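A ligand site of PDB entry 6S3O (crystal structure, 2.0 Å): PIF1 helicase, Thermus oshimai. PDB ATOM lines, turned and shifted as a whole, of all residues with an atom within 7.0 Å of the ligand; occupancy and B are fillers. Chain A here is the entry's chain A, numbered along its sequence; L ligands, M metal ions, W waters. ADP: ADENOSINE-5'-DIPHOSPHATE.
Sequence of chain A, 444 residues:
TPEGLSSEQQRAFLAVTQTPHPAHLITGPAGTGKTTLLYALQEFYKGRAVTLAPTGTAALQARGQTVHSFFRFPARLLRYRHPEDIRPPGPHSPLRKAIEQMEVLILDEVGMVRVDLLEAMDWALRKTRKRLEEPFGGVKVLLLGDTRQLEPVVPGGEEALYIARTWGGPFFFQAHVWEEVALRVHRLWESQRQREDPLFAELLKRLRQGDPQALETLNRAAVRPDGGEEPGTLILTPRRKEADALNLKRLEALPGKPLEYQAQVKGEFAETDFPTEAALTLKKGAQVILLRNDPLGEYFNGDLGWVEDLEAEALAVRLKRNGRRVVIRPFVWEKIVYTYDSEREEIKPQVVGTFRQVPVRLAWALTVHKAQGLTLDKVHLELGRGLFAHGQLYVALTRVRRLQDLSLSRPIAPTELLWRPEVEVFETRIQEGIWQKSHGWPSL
OE1 of Gln 9 is in hydrogen-bond range of N6 of the ligand (2.7 Å). O3B of the ligand sits at hydrogen-bond distance from N of Lys 34 (3.3 Å). The side-chain amino group (NZ) of Lys 34 is in salt-bridge range of an oxygen (O2B) of the ligand (2.7 Å). The backbone NH (N) of Thr 35 sits at hydrogen-bond distance from an oxygen (O3B) of the ligand. OG1 of Thr 35 is in hydrogen-bond range of O3B of the ligand (2.9 Å). N6 of the ligand lies within hydrogen-bond range of O of Gly 4, at 2.9 Å. The backbone NH (N) of Thr 32 lies within hydrogen-bond range of an oxygen (O2B) of the ligand (3.0 Å). The backbone NH (N) of Thr 36 lies within hydrogen-bond range of an oxygen (O2A) of the ligand, at 3.0 Å. The side-chain hydroxyl (OG1) of Thr 36 is in hydrogen-bond range of a nitrogen (N7) of the ligand (3.2 Å). An oxygen (O3A) of the ligand sits at hydrogen-bond distance from the backbone NH (N) of Gly 33 (3.0 Å). The backbone NH (N) of Gly 31 is in hydrogen-bond range of an oxygen (O2B) of the ligand (3.1 Å).
The side-chain amide oxygen (OE1) of Gln 9 lies within hydrogen-bond range of the backbone NH (N) of Ser 6 (2.9 Å). The side-chain amino group of Lys 34 is in hydrogen-bond range of the backbone carbonyl oxygen of Pro 29 (3.0 Å). The side-chain amino group (NZ) of Lys 34 is in hydrogen-bond range of the backbone carbonyl oxygen (O) of Gly 28 (3.0 Å). O of Leu 188 sits at hydrogen-bond distance from OG1 of Thr 32 (3.3 Å). The side-chain hydroxyl (OG1) of Thr 36 is in hydrogen-bond range of the backbone carbonyl oxygen (O) of Gly 33. The backbone NH of Gln 192 lies within hydrogen-bond range of the backbone carbonyl oxygen of Gly 31 (2.8 Å).
CA of Leu 5 touches N6 of the ligand, 3.6 Å away. Ser 6 touches the ligand (N to N6, 3.6 Å). Pro 29 touches the ligand. C of Ala 30 touches O2B of the ligand, 3.8 Å away. OE1 of Gln 192 touches C4' of the ligand, 3.9 Å away. Within 4 Å of the ligand: Gly 4, Leu 5, Ser 6, Gln 9, Pro 29, Ala 30, Gly 31, Thr 32, Gly 33, Lys 34, Thr 35, Thr 36 and Gln 192.
Water W1 bridges NE2 of Gln 61 (2.8 Å) and O1A of the ligand (3.0 Å).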
ATOM      1  N   GLY A   4      19.970  -5.281 -23.022  1.00  0.00           N
ATOM      2  CA  GLY A   4      19.038  -5.130 -21.912  1.00  0.00           C
ATOM      3  C   GLY A   4      17.803  -4.302 -22.255  1.00  0.00           C
ATOM      4  O   GLY A   4      17.152  -3.754 -21.361  1.00  0.00           O
ATOM      5  N   LEU A   5      17.500  -4.201 -23.540  1.00  0.00           N
ATOM      6  CA  LEU A   5      16.347  -3.449 -23.990  1.00  0.00           C
ATOM      7  C   LEU A   5      15.108  -4.330 -24.016  1.00  0.00           C
ATOM      8  O   LEU A   5      15.188  -5.549 -24.138  1.00  0.00           O
ATOM      9  CB  LEU A   5      16.604  -2.877 -25.381  1.00  0.00           C
ATOM     10  CG  LEU A   5      17.823  -1.963 -25.542  1.00  0.00           C
ATOM     11  CD1 LEU A   5      17.922  -1.457 -26.967  1.00  0.00           C
ATOM     12  CD2 LEU A   5      17.770  -0.798 -24.569  1.00  0.00           C
ATOM     13  N   SER A   6      13.945  -3.691 -23.890  1.00  0.00           N
ATOM     14  CA  SER A   6      12.717  -4.417 -24.154  1.00  0.00           C
ATOM     15  C   SER A   6      12.600  -4.706 -25.647  1.00  0.00           C
ATOM     16  O   SER A   6      13.404  -4.249 -26.459  1.00  0.00           O
ATOM     17  CB  SER A   6      11.503  -3.622 -23.655  1.00  0.00           C
ATOM     18  OG  SER A   6      11.395  -2.381 -24.346  1.00  0.00           O
ATOM     19  N   GLN A   9      11.982  -1.470 -27.467  1.00  0.00           N
ATOM     20  CA  GLN A   9      13.198  -0.662 -27.540  1.00  0.00           C
ATOM     21  C   GLN A   9      14.207  -1.267 -28.514  1.00  0.00           C
ATOM     22  O   GLN A   9      14.892  -0.535 -29.240  1.00  0.00           O
ATOM     23  CB  GLN A   9      13.820  -0.501 -26.150  1.00  0.00           C
ATOM     24  CG  GLN A   9      13.015   0.370 -25.208  1.00  0.00           C
ATOM     25  CD  GLN A   9      13.343   0.114 -23.759  1.00  0.00           C
ATOM     26  OE1 GLN A   9      14.069  -0.821 -23.432  1.00  0.00           O
ATOM     27  NE2 GLN A   9      12.786   0.922 -22.869  1.00  0.00           N
ATOM     28  N   GLY A  28       7.771   9.056 -27.973  1.00  0.00           N
ATOM     29  CA  GLY A  28       6.812   8.405 -27.107  1.00  0.00           C
ATOM     30  C   GLY A  28       6.656   9.191 -25.819  1.00  0.00           C
ATOM     31  O   GLY A  28       7.466  10.067 -25.514  1.00  0.00           O
ATOM     32  N   PRO A  29       5.610   8.904 -25.052  1.00  0.00           N
ATOM     33  CA  PRO A  29       5.396   9.619 -23.788  1.00  0.00           C
ATOM     34  C   PRO A  29       6.522   9.385 -22.797  1.00  0.00           C
ATOM     35  O   PRO A  29       7.396   8.530 -22.990  1.00  0.00           O
ATOM     36  CB  PRO A  29       4.065   9.053 -23.262  1.00  0.00           C
ATOM     37  CG  PRO A  29       3.391   8.474 -24.470  1.00  0.00           C
ATOM     38  CD  PRO A  29       4.504   7.980 -25.359  1.00  0.00           C
ATOM     39  N   ALA A  30       6.482  10.136 -21.701  1.00  0.00           N
ATOM     40  CA  ALA A  30       7.487   9.987 -20.660  1.00  0.00           C
ATOM     41  C   ALA A  30       7.433   8.592 -20.049  1.00  0.00           C
ATOM     42  O   ALA A  30       6.367   7.973 -19.960  1.00  0.00           O
ATOM     43  CB  ALA A  30       7.292  11.045 -19.576  1.00  0.00           C
ATOM     44  N   GLY A  31       8.587   8.094 -19.611  1.00  0.00           N
ATOM     45  CA  GLY A  31       8.664   6.773 -19.031  1.00  0.00           C
ATOM     46  C   GLY A  31       8.591   5.637 -20.020  1.00  0.00           C
ATOM     47  O   GLY A  31       8.300   4.502 -19.623  1.00  0.00           O
ATOM     48  N   THR A  32       8.848   5.899 -21.297  1.00  0.00           N
ATOM     49  CA  THR A  32       8.696   4.900 -22.349  1.00  0.00           C
ATOM     50  C   THR A  32      10.026   4.254 -22.747  1.00  0.00           C
ATOM     51  O   THR A  32      10.027   3.287 -23.511  1.00  0.00           O
ATOM     52  CB  THR A  32       8.011   5.539 -23.574  1.00  0.00           C
ATOM     53  OG1 THR A  32       7.322   4.530 -24.328  1.00  0.00           O
ATOM     54  CG2 THR A  32       9.007   6.257 -24.471  1.00  0.00           C
ATOM     55  N   GLY A  33      11.143   4.748 -22.216  1.00  0.00           N
ATOM     56  CA  GLY A  33      12.441   4.138 -22.477  1.00  0.00           C
ATOM     57  C   GLY A  33      13.349   4.931 -23.391  1.00  0.00           C
ATOM     58  O   GLY A  33      14.363   4.384 -23.831  1.00  0.00           O
ATOM     59  N   LYS A  34      13.001   6.175 -23.712  1.00  0.00           N
ATOM     60  CA  LYS A  34      13.817   6.961 -24.634  1.00  0.00           C
ATOM     61  C   LYS A  34      15.228   7.149 -24.113  1.00  0.00           C
ATOM     62  O   LYS A  34      16.197   6.971 -24.858  1.00  0.00           O
ATOM     63  CB  LYS A  34      13.152   8.328 -24.873  1.00  0.00           C
ATOM     64  CG  LYS A  34      12.352   8.420 -26.159  1.00  0.00           C
ATOM     65  CD  LYS A  34      10.954   8.964 -25.910  1.00  0.00           C
ATOM     66  CE  LYS A  34      10.966  10.117 -24.914  1.00  0.00           C
ATOM     67  NZ  LYS A  34       9.983   9.881 -23.806  1.00  0.00           N
ATOM     68  N   THR A  35      15.372   7.477 -22.827  1.00  0.00           N
ATOM     69  CA  THR A  35      16.698   7.756 -22.270  1.00  0.00           C
ATOM     70  C   THR A  35      17.560   6.493 -22.211  1.00  0.00           C
ATOM     71  O   THR A  35      18.741   6.533 -22.559  1.00  0.00           O
ATOM     72  CB  THR A  35      16.560   8.382 -20.891  1.00  0.00           C
ATOM     73  OG1 THR A  35      15.858   9.625 -20.989  1.00  0.00           O
ATOM     74  CG2 THR A  35      17.931   8.631 -20.274  1.00  0.00           C
ATOM     75  N   THR A  36      16.976   5.368 -21.783  1.00  0.00           N
ATOM     76  CA  THR A  36      17.758   4.146 -21.708  1.00  0.00           C
ATOM     77  C   THR A  36      18.088   3.613 -23.096  1.00  0.00           C
ATOM     78  O   THR A  36      19.126   2.956 -23.280  1.00  0.00           O
ATOM     79  CB  THR A  36      17.022   3.090 -20.880  1.00  0.00           C
ATOM     80  OG1 THR A  36      15.747   2.816 -21.478  1.00  0.00           O
ATOM     81  CG2 THR A  36      16.813   3.583 -19.458  1.00  0.00           C
ATOM     82  N   LEU A  37      17.250   3.906 -24.088  1.00  0.00           N
ATOM     83  CA  LEU A  37      17.596   3.604 -25.476  1.00  0.00           C
ATOM     84  C   LEU A  37      18.755   4.475 -25.936  1.00  0.00           C
ATOM     85  O   LEU A  37      19.644   4.014 -26.666  1.00  0.00           O
ATOM     86  CB  LEU A  37      16.382   3.795 -26.374  1.00  0.00           C
ATOM     87  CG  LEU A  37      16.506   3.521 -27.868  1.00  0.00           C
ATOM     88  CD1 LEU A  37      17.152   2.168 -28.143  1.00  0.00           C
ATOM     89  CD2 LEU A  37      15.115   3.580 -28.501  1.00  0.00           C
ATOM     90  N   LEU A  38      18.760   5.746 -25.530  1.00  0.00           N
ATOM     91  CA  LEU A  38      19.883   6.633 -25.845  1.00  0.00           C
ATOM     92  C   LEU A  38      21.203   6.103 -25.282  1.00  0.00           C
ATOM     93  O   LEU A  38      22.223   6.127 -25.970  1.00  0.00           O
ATOM     94  CB  LEU A  38      19.570   8.033 -25.296  1.00  0.00           C
ATOM     95  CG  LEU A  38      20.515   9.208 -25.577  1.00  0.00           C
ATOM     96  CD1 LEU A  38      19.726  10.500 -25.620  1.00  0.00           C
ATOM     97  CD2 LEU A  38      21.561   9.294 -24.501  1.00  0.00           C
ATOM     98  N   TYR A  39      21.185   5.607 -24.044  1.00  0.00           N
ATOM     99  CA  TYR A  39      22.402   5.011 -23.484  1.00  0.00           C
ATOM    100  C   TYR A  39      22.879   3.827 -24.319  1.00  0.00           C
ATOM    101  O   TYR A  39      24.084   3.654 -24.546  1.00  0.00           O
ATOM    102  CB  TYR A  39      22.156   4.576 -22.036  1.00  0.00           C
ATOM    103  CG  TYR A  39      21.813   5.703 -21.092  1.00  0.00           C
ATOM    104  CD1 TYR A  39      22.096   7.027 -21.404  1.00  0.00           C
ATOM    105  CD2 TYR A  39      21.214   5.434 -19.865  1.00  0.00           C
ATOM    106  CE1 TYR A  39      21.773   8.055 -20.531  1.00  0.00           C
ATOM    107  CE2 TYR A  39      20.888   6.452 -18.983  1.00  0.00           C
ATOM    108  CZ  TYR A  39      21.173   7.757 -19.325  1.00  0.00           C
ATOM    109  OH  TYR A  39      20.858   8.773 -18.451  1.00  0.00           O
ATOM    110  N   GLN A  61      20.802  14.510 -18.079  1.00  0.00           N
ATOM    111  CA  GLN A  61      20.157  13.201 -18.158  1.00  0.00           C
ATOM    112  C   GLN A  61      20.584  12.423 -19.401  1.00  0.00           C
ATOM    113  O   GLN A  61      20.621  11.182 -19.379  1.00  0.00           O
ATOM    114  CB  GLN A  61      18.638  13.370 -18.119  1.00  0.00           C
ATOM    115  CG  GLN A  61      17.835  12.064 -18.180  1.00  0.00           C
ATOM    116  CD  GLN A  61      17.812  11.320 -16.859  1.00  0.00           C
ATOM    117  OE1 GLN A  61      18.363  11.777 -15.853  1.00  0.00           O
ATOM    118  NE2 GLN A  61      17.151  10.161 -16.845  1.00  0.00           N
ATOM    119  N   ASP A 108      18.567  14.652 -27.728  1.00  0.00           N
ATOM    120  CA  ASP A 108      17.522  14.263 -26.791  1.00  0.00           C
ATOM    121  C   ASP A 108      16.571  15.429 -26.534  1.00  0.00           C
ATOM    122  O   ASP A 108      16.934  16.601 -26.700  1.00  0.00           O
ATOM    123  CB  ASP A 108      18.119  13.773 -25.477  1.00  0.00           C
ATOM    124  CG  ASP A 108      17.168  12.873 -24.688  1.00  0.00           C
ATOM    125  OD1 ASP A 108      16.073  12.547 -25.199  1.00  0.00           O
ATOM    126  OD2 ASP A 108      17.529  12.480 -23.563  1.00  0.00           O
ATOM    127  N   GLU A 109      15.351  15.097 -26.121  1.00  0.00           N
ATOM    128  CA  GLU A 109      14.308  16.071 -25.817  1.00  0.00           C
ATOM    129  C   GLU A 109      14.098  17.052 -26.975  1.00  0.00           C
ATOM    130  O   GLU A 109      14.049  18.273 -26.796  1.00  0.00           O
ATOM    131  CB  GLU A 109      14.609  16.820 -24.517  1.00  0.00           C
ATOM    132  CG  GLU A 109      14.578  15.940 -23.262  1.00  0.00           C
ATOM    133  CD  GLU A 109      13.174  15.621 -22.795  1.00  0.00           C
ATOM    134  OE1 GLU A 109      13.035  15.030 -21.697  1.00  0.00           O
ATOM    135  OE2 GLU A 109      12.206  15.967 -23.505  1.00  0.00           O
ATOM    136  N   LEU A 188       7.578   4.499 -29.363  1.00  0.00           N
ATOM    137  CA  LEU A 188       7.568   3.651 -28.185  1.00  0.00           C
ATOM    138  C   LEU A 188       6.250   3.881 -27.459  1.00  0.00           C
ATOM    139  O   LEU A 188       5.872   5.024 -27.196  1.00  0.00           O
ATOM    140  CB  LEU A 188       8.760   3.939 -27.267  1.00  0.00           C
ATOM    141  CG  LEU A 188      10.144   3.907 -27.912  1.00  0.00           C
ATOM    142  CD1 LEU A 188      11.183   4.530 -26.995  1.00  0.00           C
ATOM    143  CD2 LEU A 188      10.528   2.475 -28.273  1.00  0.00           C
ATOM    144  N   SER A 191       4.979   2.139 -21.439  1.00  0.00           N
ATOM    145  CA  SER A 191       5.513   3.087 -20.474  1.00  0.00           C
ATOM    146  C   SER A 191       5.529   2.485 -19.079  1.00  0.00           C
ATOM    147  O   SER A 191       4.753   1.568 -18.765  1.00  0.00           O
ATOM    148  CB  SER A 191       4.681   4.382 -20.454  1.00  0.00           C
ATOM    149  OG  SER A 191       3.357   4.105 -20.040  1.00  0.00           O
ATOM    150  N   GLN A 192       6.435   3.002 -18.253  1.00  0.00           N
ATOM    151  CA  GLN A 192       6.437   2.684 -16.822  1.00  0.00           C
ATOM    152  C   GLN A 192       5.059   2.909 -16.211  1.00  0.00           C
ATOM    153  O   GLN A 192       4.565   2.075 -15.438  1.00  0.00           O
ATOM    154  CB  GLN A 192       7.493   3.531 -16.120  1.00  0.00           C
ATOM    155  CG  GLN A 192       7.591   3.325 -14.615  1.00  0.00           C
ATOM    156  CD  GLN A 192       8.667   4.204 -13.989  1.00  0.00           C
ATOM    157  OE1 GLN A 192       8.936   5.306 -14.463  1.00  0.00           O
ATOM    158  NE2 GLN A 192       9.291   3.695 -12.925  1.00  0.00           N
ATOM    159  N   ARG A 195       2.450   0.259 -16.306  1.00  0.00           N
ATOM    160  CA  ARG A 195       2.599  -0.794 -15.305  1.00  0.00           C
ATOM    161  C   ARG A 195       2.272  -0.284 -13.897  1.00  0.00           C
ATOM    162  O   ARG A 195       1.668  -1.002 -13.103  1.00  0.00           O
ATOM    163  CB  ARG A 195       4.003  -1.371 -15.349  1.00  0.00           C
ATOM    164  CG  ARG A 195       4.385  -1.965 -16.688  1.00  0.00           C
ATOM    165  CD  ARG A 195       5.846  -2.368 -16.725  1.00  0.00           C
ATOM    166  NE  ARG A 195       6.647  -1.558 -15.811  1.00  0.00           N
ATOM    167  CZ  ARG A 195       7.637  -0.748 -16.196  1.00  0.00           C
ATOM    168  NH1 ARG A 195       7.936  -0.634 -17.489  1.00  0.00           N
ATOM    169  NH2 ARG A 195       8.312  -0.039 -15.301  1.00  0.00           N
HETATM  170  PB  ADP L   1      11.861   8.299 -20.891  1.00  0.00           P
HETATM  171  O1B ADP L   1      11.532   9.177 -19.697  1.00  0.00           O
HETATM  172  O2B ADP L   1      10.729   8.128 -21.865  1.00  0.00           O
HETATM  173  O3B ADP L   1      13.180   8.612 -21.560  1.00  0.00           O
HETATM  174  PA  ADP L   1      13.334   6.344 -19.389  1.00  0.00           P
HETATM  175  O1A ADP L   1      13.635   7.372 -18.336  1.00  0.00           O
HETATM  176  O2A ADP L   1      14.414   5.848 -20.325  1.00  0.00           O
HETATM  177  O3A ADP L   1      12.060   6.826 -20.270  1.00  0.00           O
HETATM  178  O5' ADP L   1      12.688   5.050 -18.682  1.00  0.00           O
HETATM  179  C5' ADP L   1      11.763   5.212 -17.601  1.00  0.00           C
HETATM  180  C4' ADP L   1      12.161   4.267 -16.474  1.00  0.00           C
HETATM  181  O4' ADP L   1      12.011   2.917 -16.892  1.00  0.00           O
HETATM  182  C3' ADP L   1      13.622   4.488 -16.126  1.00  0.00           C
HETATM  183  O3' ADP L   1      13.745   4.864 -14.751  1.00  0.00           O
HETATM  184  C2' ADP L   1      14.319   3.166 -16.368  1.00  0.00           C
HETATM  185  O2' ADP L   1      15.022   2.780 -15.193  1.00  0.00           O
HETATM  186  C1' ADP L   1      13.213   2.162 -16.687  1.00  0.00           C
HETATM  187  N9  ADP L   1      13.527   1.400 -17.922  1.00  0.00           N
HETATM  188  C8  ADP L   1      13.155   1.762 -19.173  1.00  0.00           C
HETATM  189  N7  ADP L   1      13.589   0.862 -20.090  1.00  0.00           N
HETATM  190  C5  ADP L   1      14.253  -0.104 -19.430  1.00  0.00           C
HETATM  191  C6  ADP L   1      14.957  -1.349 -19.802  1.00  0.00           C
HETATM  192  N6  ADP L   1      15.049  -1.762 -21.092  1.00  0.00           N
HETATM  193  N1  ADP L   1      15.520  -2.078 -18.809  1.00  0.00           N
HETATM  194  C2  ADP L   1      15.446  -1.688 -17.525  1.00  0.00           C
HETATM  195  N3  ADP L   1      14.820  -0.568 -17.121  1.00  0.00           N
HETATM  196  C4  ADP L   1      14.209   0.253 -18.009  1.00  0.00           C
HETATM  197 MG    MG M   1      13.871  11.145 -21.925  1.00  0.00          MG
HETATM  198  O   HOH W   1      16.165   7.505 -16.749  1.00  0.00           O
HETATM  199  O   HOH W   2      11.821  11.919 -20.211  1.00  0.00           O
